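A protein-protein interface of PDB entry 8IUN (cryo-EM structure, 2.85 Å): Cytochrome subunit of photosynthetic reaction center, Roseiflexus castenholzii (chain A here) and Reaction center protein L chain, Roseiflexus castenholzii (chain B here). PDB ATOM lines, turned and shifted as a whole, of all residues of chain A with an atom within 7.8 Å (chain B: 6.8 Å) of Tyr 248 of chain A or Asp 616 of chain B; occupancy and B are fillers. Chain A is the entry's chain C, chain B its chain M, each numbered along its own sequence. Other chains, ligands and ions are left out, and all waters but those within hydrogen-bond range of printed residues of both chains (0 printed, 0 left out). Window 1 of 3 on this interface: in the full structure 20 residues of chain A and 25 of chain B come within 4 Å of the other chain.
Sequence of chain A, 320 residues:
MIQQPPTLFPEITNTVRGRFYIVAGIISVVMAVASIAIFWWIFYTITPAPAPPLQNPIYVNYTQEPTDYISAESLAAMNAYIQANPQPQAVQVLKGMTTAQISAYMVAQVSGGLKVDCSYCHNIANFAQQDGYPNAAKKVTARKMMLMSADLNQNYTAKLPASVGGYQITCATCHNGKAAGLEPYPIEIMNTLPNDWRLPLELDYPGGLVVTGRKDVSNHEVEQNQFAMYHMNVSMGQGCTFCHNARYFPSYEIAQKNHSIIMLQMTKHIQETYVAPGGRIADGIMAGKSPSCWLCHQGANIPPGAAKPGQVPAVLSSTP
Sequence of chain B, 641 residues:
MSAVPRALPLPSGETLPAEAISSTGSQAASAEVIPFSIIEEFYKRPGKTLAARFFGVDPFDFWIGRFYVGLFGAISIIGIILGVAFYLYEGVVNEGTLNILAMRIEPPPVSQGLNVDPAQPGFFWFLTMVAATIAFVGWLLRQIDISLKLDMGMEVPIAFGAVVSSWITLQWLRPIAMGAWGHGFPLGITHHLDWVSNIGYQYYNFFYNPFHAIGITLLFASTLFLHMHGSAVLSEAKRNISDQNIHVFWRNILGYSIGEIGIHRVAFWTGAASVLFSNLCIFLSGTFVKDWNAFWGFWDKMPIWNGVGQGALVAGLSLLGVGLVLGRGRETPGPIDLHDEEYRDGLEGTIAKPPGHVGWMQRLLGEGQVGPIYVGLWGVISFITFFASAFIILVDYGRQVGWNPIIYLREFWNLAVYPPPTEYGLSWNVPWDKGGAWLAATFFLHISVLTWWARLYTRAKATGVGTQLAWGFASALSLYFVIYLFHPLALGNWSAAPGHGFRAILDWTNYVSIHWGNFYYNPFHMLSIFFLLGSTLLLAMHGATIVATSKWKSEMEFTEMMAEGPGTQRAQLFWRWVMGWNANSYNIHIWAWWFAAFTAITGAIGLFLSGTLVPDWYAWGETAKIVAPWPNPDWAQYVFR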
ATOM      1  N   THR A 212      16.677  -7.473   3.905  1.00  0.00           N
ATOM      2  CA  THR A 212      16.346  -6.451   4.892  1.00  0.00           C
ATOM      3  C   THR A 212      17.581  -6.039   5.684  1.00  0.00           C
ATOM      4  O   THR A 212      18.239  -6.879   6.305  1.00  0.00           O
ATOM      5  CB  THR A 212      15.253  -6.943   5.835  1.00  0.00           C
ATOM      6  OG1 THR A 212      14.018  -7.046   5.119  1.00  0.00           O
ATOM      7  CG2 THR A 212      15.075  -5.978   6.989  1.00  0.00           C
ATOM      8  N   GLY A 213      17.883  -4.741   5.667  1.00  0.00           N
ATOM      9  CA  GLY A 213      18.947  -4.176   6.466  1.00  0.00           C
ATOM     10  C   GLY A 213      20.345  -4.404   5.948  1.00  0.00           C
ATOM     11  O   GLY A 213      21.304  -4.108   6.665  1.00  0.00           O
ATOM     12  N   ARG A 214      20.498  -4.902   4.727  1.00  0.00           N
ATOM     13  CA  ARG A 214      21.800  -5.287   4.199  1.00  0.00           C
ATOM     14  C   ARG A 214      22.399  -4.138   3.403  1.00  0.00           C
ATOM     15  O   ARG A 214      21.739  -3.574   2.525  1.00  0.00           O
ATOM     16  CB  ARG A 214      21.676  -6.533   3.329  1.00  0.00           C
ATOM     17  CG  ARG A 214      21.373  -7.786   4.103  1.00  0.00           C
ATOM     18  CD  ARG A 214      22.215  -8.921   3.596  1.00  0.00           C
ATOM     19  NE  ARG A 214      21.618  -9.583   2.447  1.00  0.00           N
ATOM     20  CZ  ARG A 214      22.292 -10.319   1.577  1.00  0.00           C
ATOM     21  NH1 ARG A 214      23.605 -10.448   1.653  1.00  0.00           N
ATOM     22  NH2 ARG A 214      21.634 -10.935   0.602  1.00  0.00           N
ATOM     23  N   CYS A 243       2.040 -16.070   4.150  1.00  0.00           N
ATOM     24  CA  CYS A 243       3.320 -16.495   4.758  1.00  0.00           C
ATOM     25  C   CYS A 243       3.958 -15.388   5.623  1.00  0.00           C
ATOM     26  O   CYS A 243       4.871 -15.741   6.338  1.00  0.00           O
ATOM     27  CB  CYS A 243       4.296 -16.968   3.679  1.00  0.00           C
ATOM     28  SG  CYS A 243       3.847 -18.254   2.461  1.00  0.00           S
ATOM     29  N   HIS A 244       3.490 -14.123   5.635  1.00  0.00           N
ATOM     30  CA  HIS A 244       4.142 -13.010   6.305  1.00  0.00           C
ATOM     31  C   HIS A 244       3.173 -12.217   7.163  1.00  0.00           C
ATOM     32  O   HIS A 244       1.976 -12.154   6.887  1.00  0.00           O
ATOM     33  CB  HIS A 244       4.781 -12.044   5.296  1.00  0.00           C
ATOM     34  CG  HIS A 244       6.015 -12.577   4.642  1.00  0.00           C
ATOM     35  ND1 HIS A 244       7.240 -12.579   5.266  1.00  0.00           N
ATOM     36  CD2 HIS A 244       6.212 -13.121   3.421  1.00  0.00           C
ATOM     37  CE1 HIS A 244       8.139 -13.107   4.460  1.00  0.00           C
ATOM     38  NE2 HIS A 244       7.543 -13.442   3.332  1.00  0.00           N
ATOM     39  N   ASN A 245       3.720 -11.624   8.220  1.00  0.00           N
ATOM     40  CA  ASN A 245       3.139 -10.456   8.867  1.00  0.00           C
ATOM     41  C   ASN A 245       3.789  -9.239   8.222  1.00  0.00           C
ATOM     42  O   ASN A 245       4.994  -9.026   8.360  1.00  0.00           O
ATOM     43  CB  ASN A 245       3.382 -10.494  10.371  1.00  0.00           C
ATOM     44  CG  ASN A 245       2.547  -9.490  11.132  1.00  0.00           C
ATOM     45  OD1 ASN A 245       2.216  -8.431  10.623  1.00  0.00           O
ATOM     46  ND2 ASN A 245       2.205  -9.823  12.362  1.00  0.00           N
ATOM     47  N   ALA A 246       2.996  -8.447   7.503  1.00  0.00           N
ATOM     48  CA  ALA A 246       3.537  -7.417   6.631  1.00  0.00           C
ATOM     49  C   ALA A 246       4.154  -6.249   7.384  1.00  0.00           C
ATOM     50  O   ALA A 246       4.745  -5.376   6.743  1.00  0.00           O
ATOM     51  CB  ALA A 246       2.447  -6.915   5.691  1.00  0.00           C
ATOM     52  N   ARG A 247       4.023  -6.191   8.710  1.00  0.00           N
ATOM     53  CA  ARG A 247       4.732  -5.173   9.474  1.00  0.00           C
ATOM     54  C   ARG A 247       6.191  -5.532   9.716  1.00  0.00           C
ATOM     55  O   ARG A 247       6.974  -4.652  10.081  1.00  0.00           O
ATOM     56  CB  ARG A 247       4.020  -4.901  10.803  1.00  0.00           C
ATOM     57  CG  ARG A 247       4.375  -5.812  11.956  1.00  0.00           C
ATOM     58  CD  ARG A 247       3.742  -5.300  13.238  1.00  0.00           C
ATOM     59  NE  ARG A 247       4.050  -6.128  14.397  1.00  0.00           N
ATOM     60  CZ  ARG A 247       3.687  -5.848  15.641  1.00  0.00           C
ATOM     61  NH1 ARG A 247       2.986  -4.767  15.929  1.00  0.00           N
ATOM     62  NH2 ARG A 247       4.043  -6.669  16.620  1.00  0.00           N
ATOM     63  N   TYR A 248       6.576  -6.789   9.507  1.00  0.00           N
ATOM     64  CA  TYR A 248       7.982  -7.186   9.522  1.00  0.00           C
ATOM     65  C   TYR A 248       8.113  -8.446   8.677  1.00  0.00           C
ATOM     66  O   TYR A 248       7.696  -9.522   9.111  1.00  0.00           O
ATOM     67  CB  TYR A 248       8.462  -7.424  10.942  1.00  0.00           C
ATOM     68  CG  TYR A 248       9.959  -7.366  11.109  1.00  0.00           C
ATOM     69  CD1 TYR A 248      10.699  -6.343  10.541  1.00  0.00           C
ATOM     70  CD2 TYR A 248      10.627  -8.315  11.859  1.00  0.00           C
ATOM     71  CE1 TYR A 248      12.055  -6.280  10.699  1.00  0.00           C
ATOM     72  CE2 TYR A 248      11.983  -8.257  12.025  1.00  0.00           C
ATOM     73  CZ  TYR A 248      12.694  -7.238  11.442  1.00  0.00           C
ATOM     74  OH  TYR A 248      14.054  -7.177  11.605  1.00  0.00           O
ATOM     75  N   PHE A 249       8.673  -8.313   7.483  1.00  0.00           N
ATOM     76  CA  PHE A 249       8.833  -9.446   6.574  1.00  0.00           C
ATOM     77  C   PHE A 249       9.881 -10.470   7.017  1.00  0.00           C
ATOM     78  O   PHE A 249       9.775 -11.637   6.623  1.00  0.00           O
ATOM     79  CB  PHE A 249       9.146  -8.947   5.163  1.00  0.00           C
ATOM     80  CG  PHE A 249       7.950  -8.409   4.439  1.00  0.00           C
ATOM     81  CD1 PHE A 249       6.893  -9.232   4.125  1.00  0.00           C
ATOM     82  CD2 PHE A 249       7.884  -7.083   4.067  1.00  0.00           C
ATOM     83  CE1 PHE A 249       5.797  -8.745   3.468  1.00  0.00           C
ATOM     84  CE2 PHE A 249       6.789  -6.597   3.408  1.00  0.00           C
ATOM     85  CZ  PHE A 249       5.748  -7.431   3.111  1.00  0.00           C
ATOM     86  N   PRO A 250      10.916 -10.105   7.784  1.00  0.00           N
ATOM     87  CA  PRO A 250      11.813 -11.138   8.330  1.00  0.00           C
ATOM     88  C   PRO A 250      11.179 -12.081   9.349  1.00  0.00           C
ATOM     89  O   PRO A 250      11.791 -13.106   9.661  1.00  0.00           O
ATOM     90  CB  PRO A 250      12.933 -10.317   8.970  1.00  0.00           C
ATOM     91  CG  PRO A 250      12.975  -9.111   8.189  1.00  0.00           C
ATOM     92  CD  PRO A 250      11.565  -8.784   7.846  1.00  0.00           C
ATOM     93  N   SER A 251      10.000 -11.775   9.881  1.00  0.00           N
ATOM     94  CA  SER A 251       9.431 -12.552  10.977  1.00  0.00           C
ATOM     95  C   SER A 251       8.980 -13.938  10.520  1.00  0.00           C
ATOM     96  O   SER A 251       8.501 -14.116   9.399  1.00  0.00           O
ATOM     97  CB  SER A 251       8.256 -11.795  11.586  1.00  0.00           C
ATOM     98  OG  SER A 251       7.716 -12.488  12.692  1.00  0.00           O
ATOM     99  N   TYR A 252       9.112 -14.921  11.411  1.00  0.00           N
ATOM    100  CA  TYR A 252       8.752 -16.312  11.146  1.00  0.00           C
ATOM    101  C   TYR A 252       7.562 -16.773  11.983  1.00  0.00           C
ATOM    102  O   TYR A 252       7.531 -17.904  12.462  1.00  0.00           O
ATOM    103  CB  TYR A 252       9.935 -17.241  11.409  1.00  0.00           C
ATOM    104  CG  TYR A 252      10.791 -17.547  10.207  1.00  0.00           C
ATOM    105  CD1 TYR A 252      10.465 -18.577   9.346  1.00  0.00           C
ATOM    106  CD2 TYR A 252      11.935 -16.819   9.944  1.00  0.00           C
ATOM    107  CE1 TYR A 252      11.241 -18.861   8.253  1.00  0.00           C
ATOM    108  CE2 TYR A 252      12.715 -17.098   8.855  1.00  0.00           C
ATOM    109  CZ  TYR A 252      12.366 -18.121   8.014  1.00  0.00           C
ATOM    110  OH  TYR A 252      13.145 -18.402   6.922  1.00  0.00           O
ATOM    111  N   GLU A 253       6.566 -15.915  12.169  1.00  0.00           N
ATOM    112  CA  GLU A 253       5.452 -16.216  13.059  1.00  0.00           C
ATOM    113  C   GLU A 253       4.284 -16.909  12.367  1.00  0.00           C
ATOM    114  O   GLU A 253       3.321 -17.278  13.043  1.00  0.00           O
ATOM    115  CB  GLU A 253       4.960 -14.938  13.730  1.00  0.00           C
ATOM    116  CG  GLU A 253       4.320 -13.961  12.782  1.00  0.00           C
ATOM    117  CD  GLU A 253       4.530 -12.531  13.204  1.00  0.00           C
ATOM    118  OE1 GLU A 253       3.737 -12.033  14.026  1.00  0.00           O
ATOM    119  OE2 GLU A 253       5.484 -11.897  12.706  1.00  0.00           O
ATOM    120  N   LYS A 257       5.680 -20.042   6.200  1.00  0.00           N
ATOM    121  CA  LYS A 257       7.025 -19.645   5.792  1.00  0.00           C
ATOM    122  C   LYS A 257       8.026 -20.786   5.975  1.00  0.00           C
ATOM    123  O   LYS A 257       8.896 -21.001   5.123  1.00  0.00           O
ATOM    124  CB  LYS A 257       7.456 -18.402   6.566  1.00  0.00           C
ATOM    125  CG  LYS A 257       8.445 -17.537   5.819  1.00  0.00           C
ATOM    126  CD  LYS A 257       8.841 -16.308   6.600  1.00  0.00           C
ATOM    127  CE  LYS A 257      10.089 -15.702   6.018  1.00  0.00           C
ATOM    128  NZ  LYS A 257      10.541 -14.532   6.784  1.00  0.00           N
ATOM    129  N   HIS B 515      13.524  -2.500   1.806  1.00  0.00           N
ATOM    130  CA  HIS B 515      14.946  -2.686   2.091  1.00  0.00           C
ATOM    131  C   HIS B 515      15.295  -2.280   3.518  1.00  0.00           C
ATOM    132  O   HIS B 515      15.961  -3.026   4.240  1.00  0.00           O
ATOM    133  CB  HIS B 515      15.770  -1.878   1.088  1.00  0.00           C
ATOM    134  CG  HIS B 515      17.231  -2.206   1.082  1.00  0.00           C
ATOM    135  ND1 HIS B 515      18.117  -1.606   0.217  1.00  0.00           N
ATOM    136  CD2 HIS B 515      17.959  -3.071   1.824  1.00  0.00           C
ATOM    137  CE1 HIS B 515      19.328  -2.083   0.428  1.00  0.00           C
ATOM    138  NE2 HIS B 515      19.260  -2.976   1.397  1.00  0.00           N
ATOM    139  N   TRP B 516      14.870  -1.090   3.936  1.00  0.00           N
ATOM    140  CA  TRP B 516      15.245  -0.548   5.242  1.00  0.00           C
ATOM    141  C   TRP B 516      14.120  -0.762   6.254  1.00  0.00           C
ATOM    142  O   TRP B 516      13.465   0.172   6.700  1.00  0.00           O
ATOM    143  CB  TRP B 516      15.601   0.930   5.119  1.00  0.00           C
ATOM    144  CG  TRP B 516      16.616   1.235   4.068  1.00  0.00           C
ATOM    145  CD1 TRP B 516      16.453   2.045   2.988  1.00  0.00           C
ATOM    146  CD2 TRP B 516      17.952   0.732   3.994  1.00  0.00           C
ATOM    147  NE1 TRP B 516      17.602   2.080   2.248  1.00  0.00           N
ATOM    148  CE2 TRP B 516      18.540   1.283   2.846  1.00  0.00           C
ATOM    149  CE3 TRP B 516      18.708  -0.132   4.788  1.00  0.00           C
ATOM    150  CZ2 TRP B 516      19.847   0.999   2.473  1.00  0.00           C
ATOM    151  CZ3 TRP B 516      19.997  -0.410   4.417  1.00  0.00           C
ATOM    152  CH2 TRP B 516      20.556   0.150   3.271  1.00  0.00           C
ATOM    153  N   GLY B 517      13.924  -2.019   6.634  1.00  0.00           N
ATOM    154  CA  GLY B 517      12.897  -2.321   7.611  1.00  0.00           C
ATOM    155  C   GLY B 517      11.513  -1.961   7.109  1.00  0.00           C
ATOM    156  O   GLY B 517      11.121  -2.286   5.989  1.00  0.00           O
ATOM    157  N   ASN B 518      10.753  -1.283   7.957  1.00  0.00           N
ATOM    158  CA  ASN B 518       9.416  -0.815   7.618  1.00  0.00           C
ATOM    159  C   ASN B 518       9.380   0.702   7.741  1.00  0.00           C
ATOM    160  O   ASN B 518       9.748   1.249   8.783  1.00  0.00           O
ATOM    161  CB  ASN B 518       8.389  -1.468   8.545  1.00  0.00           C
ATOM    162  CG  ASN B 518       6.966  -1.180   8.150  1.00  0.00           C
ATOM    163  OD1 ASN B 518       6.703  -0.479   7.184  1.00  0.00           O
ATOM    164  ND2 ASN B 518       6.034  -1.738   8.898  1.00  0.00           N
ATOM    165  N   SER B 610      17.487   7.213   6.463  1.00  0.00           N
ATOM    166  CA  SER B 610      16.889   5.885   6.347  1.00  0.00           C
ATOM    167  C   SER B 610      17.918   4.775   6.158  1.00  0.00           C
ATOM    168  O   SER B 610      17.759   3.684   6.707  1.00  0.00           O
ATOM    169  CB  SER B 610      15.888   5.872   5.202  1.00  0.00           C
ATOM    170  OG  SER B 610      15.225   4.632   5.149  1.00  0.00           O
ATOM    171  N   LEU B 613      22.155   5.678   8.935  1.00  0.00           N
ATOM    172  CA  LEU B 613      22.272   5.571  10.385  1.00  0.00           C
ATOM    173  C   LEU B 613      21.396   4.488  10.992  1.00  0.00           C
ATOM    174  O   LEU B 613      21.814   3.842  11.951  1.00  0.00           O
ATOM    175  CB  LEU B 613      21.945   6.911  11.053  1.00  0.00           C
ATOM    176  CG  LEU B 613      22.917   8.083  10.872  1.00  0.00           C
ATOM    177  CD1 LEU B 613      22.486   9.254  11.722  1.00  0.00           C
ATOM    178  CD2 LEU B 613      24.338   7.692  11.213  1.00  0.00           C
ATOM    179  N   VAL B 614      20.195   4.273  10.472  1.00  0.00           N
ATOM    180  CA  VAL B 614      19.271   3.274  10.991  1.00  0.00           C
ATOM    181  C   VAL B 614      18.931   2.304   9.868  1.00  0.00           C
ATOM    182  O   VAL B 614      18.100   2.598   9.012  1.00  0.00           O
ATOM    183  CB  VAL B 614      17.999   3.922  11.565  1.00  0.00           C
ATOM    184  CG1 VAL B 614      17.052   2.858  12.066  1.00  0.00           C
ATOM    185  CG2 VAL B 614      18.346   4.883  12.681  1.00  0.00           C
ATOM    186  N   PRO B 615      19.538   1.114   9.855  1.00  0.00           N
ATOM    187  CA  PRO B 615      19.291   0.157   8.769  1.00  0.00           C
ATOM    188  C   PRO B 615      18.008  -0.648   8.903  1.00  0.00           C
ATOM    189  O   PRO B 615      17.745  -1.496   8.046  1.00  0.00           O
ATOM    190  CB  PRO B 615      20.512  -0.759   8.861  1.00  0.00           C
ATOM    191  CG  PRO B 615      20.829  -0.766  10.299  1.00  0.00           C
ATOM    192  CD  PRO B 615      20.544   0.613  10.804  1.00  0.00           C
ATOM    193  N   ASP B 616      17.208  -0.419   9.940  1.00  0.00           N
ATOM    194  CA  ASP B 616      16.021  -1.232  10.192  1.00  0.00           C
ATOM    195  C   ASP B 616      15.134  -0.433  11.133  1.00  0.00           C
ATOM    196  O   ASP B 616      15.529  -0.170  12.271  1.00  0.00           O
ATOM    197  CB  ASP B 616      16.419  -2.569  10.797  1.00  0.00           C
ATOM    198  CG  ASP B 616      15.329  -3.596  10.724  1.00  0.00           C
ATOM    199  OD1 ASP B 616      14.147  -3.227  10.830  1.00  0.00           O
ATOM    200  OD2 ASP B 616      15.659  -4.784  10.571  1.00  0.00           O
ATOM    201  N   TRP B 617      13.952  -0.040  10.663  1.00  0.00           N
ATOM    202  CA  TRP B 617      13.129   0.873  11.444  1.00  0.00           C
ATOM    203  C   TRP B 617      12.205   0.145  12.409  1.00  0.00           C
ATOM    204  O   TRP B 617      11.871   0.690  13.465  1.00  0.00           O
ATOM    205  CB  TRP B 617      12.328   1.782  10.513  1.00  0.00           C
ATOM    206  CG  TRP B 617      13.163   2.851   9.871  1.00  0.00           C
ATOM    207  CD1 TRP B 617      13.535   2.921   8.567  1.00  0.00           C
ATOM    208  CD2 TRP B 617      13.750   3.986  10.519  1.00  0.00           C
ATOM    209  NE1 TRP B 617      14.307   4.033   8.356  1.00  0.00           N
ATOM    210  CE2 TRP B 617      14.457   4.702   9.540  1.00  0.00           C
ATOM    211  CE3 TRP B 617      13.742   4.467  11.831  1.00  0.00           C
ATOM    212  CZ2 TRP B 617      15.144   5.875   9.827  1.00  0.00           C
ATOM    213  CZ3 TRP B 617      14.423   5.626  12.114  1.00  0.00           C
ATOM    214  CH2 TRP B 617      15.115   6.318  11.118  1.00  0.00           C
ATOM    215  N   TYR B 618      11.794  -1.080  12.082  1.00  0.00           N
ATOM    216  CA  TYR B 618      10.984  -1.859  13.010  1.00  0.00           C
ATOM    217  C   TYR B 618      11.783  -2.258  14.246  1.00  0.00           C
ATOM    218  O   TYR B 618      11.284  -2.158  15.372  1.00  0.00           O
ATOM    219  CB  TYR B 618      10.424  -3.088  12.299  1.00  0.00           C
ATOM    220  CG  TYR B 618       9.617  -4.009  13.181  1.00  0.00           C
ATOM    221  CD1 TYR B 618       8.253  -3.843  13.326  1.00  0.00           C
ATOM    222  CD2 TYR B 618      10.224  -5.052  13.862  1.00  0.00           C
ATOM    223  CE1 TYR B 618       7.523  -4.683  14.124  1.00  0.00           C
ATOM    224  CE2 TYR B 618       9.505  -5.888  14.661  1.00  0.00           C
ATOM    225  CZ  TYR B 618       8.157  -5.705  14.787  1.00  0.00           C
ATOM    226  OH  TYR B 618       7.447  -6.557  15.591  1.00  0.00           O
ATOM    227  N   ALA B 619      13.023  -2.713  14.059  1.00  0.00           N
ATOM    228  CA  ALA B 619      13.872  -3.060  15.194  1.00  0.00           C
ATOM    229  C   ALA B 619      14.183  -1.840  16.055  1.00  0.00           C
ATOM    230  O   ALA B 619      14.184  -1.923  17.293  1.00  0.00           O
ATOM    231  CB  ALA B 619      15.157  -3.710  14.692  1.00  0.00           C
ATOM    232  N   TRP B 620      14.446  -0.698  15.420  1.00  0.00           N
ATOM    233  CA  TRP B 620      14.654   0.535  16.169  1.00  0.00           C
ATOM    234  C   TRP B 620      13.418   0.897  16.980  1.00  0.00           C
ATOM    235  O   TRP B 620      13.519   1.217  18.167  1.00  0.00           O
ATOM    236  CB  TRP B 620      15.024   1.674  15.218  1.00  0.00           C
ATOM    237  CG  TRP B 620      15.181   2.992  15.908  1.00  0.00           C
ATOM    238  CD1 TRP B 620      16.315   3.492  16.462  1.00  0.00           C
ATOM    239  CD2 TRP B 620      14.162   3.974  16.127  1.00  0.00           C
ATOM    240  NE1 TRP B 620      16.071   4.722  17.013  1.00  0.00           N
ATOM    241  CE2 TRP B 620      14.755   5.041  16.820  1.00  0.00           C
ATOM    242  CE3 TRP B 620      12.805   4.054  15.801  1.00  0.00           C
ATOM    243  CZ2 TRP B 620      14.042   6.171  17.195  1.00  0.00           C
ATOM    244  CZ3 TRP B 620      12.100   5.172  16.179  1.00  0.00           C
ATOM    245  CH2 TRP B 620      12.718   6.218  16.864  1.00  0.00           C
ATOM    246  N   GLY B 621      12.239   0.842  16.360  1.00  0.00           N
ATOM    247  CA  GLY B 621      11.013   1.121  17.083  1.00  0.00           C
ATOM    248  C   GLY B 621      10.733   0.146  18.201  1.00  0.00           C
ATOM    249  O   GLY B 621      10.062   0.506  19.169  1.00  0.00           O
ATOM    250  N   GLU B 622      11.212  -1.090  18.077  1.00  0.00           N
ATOM    251  CA  GLU B 622      11.118  -2.043  19.174  1.00  0.00           C
ATOM    252  C   GLU B 622      12.022  -1.671  20.337  1.00  0.00           C
ATOM    253  O   GLU B 622      11.637  -1.857  21.495  1.00  0.00           O
ATOM    254  CB  GLU B 622      11.459  -3.445  18.687  1.00  0.00           C
ATOM    255  CG  GLU B 622      10.341  -4.121  17.950  1.00  0.00           C
ATOM    256  CD  GLU B 622      10.430  -5.618  18.047  1.00  0.00           C
ATOM    257  OE1 GLU B 622      11.412  -6.184  17.527  1.00  0.00           O
ATOM    258  OE2 GLU B 622       9.528  -6.230  18.651  1.00  0.00           O
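N of Gly 213 of chain A sits at hydrogen-bond distance from O of His 515 of chain B (2.9 Å).
A ring nitrogen (NE2) of His 515 of chain B is in hydrogen-bond range of the backbone carbonyl oxygen (O) of Arg 214 of chain A.
OH of Tyr 248 of chain A sits at hydrogen-bond distance from OD2 of Asp 616 of chain B, 3.1 Å away.
ND2 of Asn 518 of chain B is in hydrogen-bond range of O of Arg 247 of chain A, 3.3 Å away.
The side-chain amide oxygen (OD1) of Asn 245 of chain A sits close to the backbone NH (N) of Arg 247 of chain A (3.5 Å).
The side-chain carboxylate of Asp 616 of chain B lies within hydrogen-bond range of the backbone NH of Ala 619 of chain B, 3.5 Å away.
N of Tyr 618 of chain B sits at hydrogen-bond distance from OD1 of Asp 616 of chain B (3.4 Å).
Among the printed residues, pairs that only touch across the chains: Gly 213 of chain A with Pro 615 of chain B (3.3 Å), Thr 212 of chain A with His 515 of chain B (3.5 Å), Arg 247 of chain A with Tyr 618 of chain B (3.6 Å), Tyr 248 of chain A with Tyr 618 of chain B (3.6 Å), Thr 212 of chain A with Asp 616 of chain B (3.8 Å) and Arg 214 of chain A with Trp 516 of chain B (3.98 Å).
Of the printed residues of chain B, Thr 212 of chain A touches His 515 and Asp 616.
Of chain B, only Asp 616 (3.1 Å) and Tyr 618 (3.6 Å) come within 4 Å of Tyr 248 of chain A.
Printed residues of chain A within 4 Å of His 515 of chain B: Thr 212 (3.5 Å), Gly 213 (2.9 Å) and Arg 214 (2.8 Å).
Printed residues of chain A within 4 Å of Pro 615 of chain B: Gly 213 (3.3 Å).
Of chain A, only Thr 212 (3.8 Å) and Tyr 248 (3.1 Å) come within 4 Å of Asp 616 of chain B.
Glu 622 of chain B touches none of the printed residues of chain A.
The nearest residue of chain B that does not touch Tyr 248 of chain A is Ala 619 of chain B (4.8 Å).
The nearest printed residue of chain A that does not touch Asn 518 of chain B is Ala 246 of chain A (4.4 Å).
Of the 15 printed residues of chain A, 5 touch a printed residue of chain B.
Hydrophobic or aromatic side chains of chain A that line the printed part of chain B: Tyr 248.
Printed residues of chain B that touch a printed residue of chain A: His 515, Trp 516, Asn 518, Pro 615, Asp 616 and Tyr 618.
Among the printed residues, no Asp or Glu carboxylate lies within 4 Å of a Lys or Arg side-chain nitrogen of the other chain.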
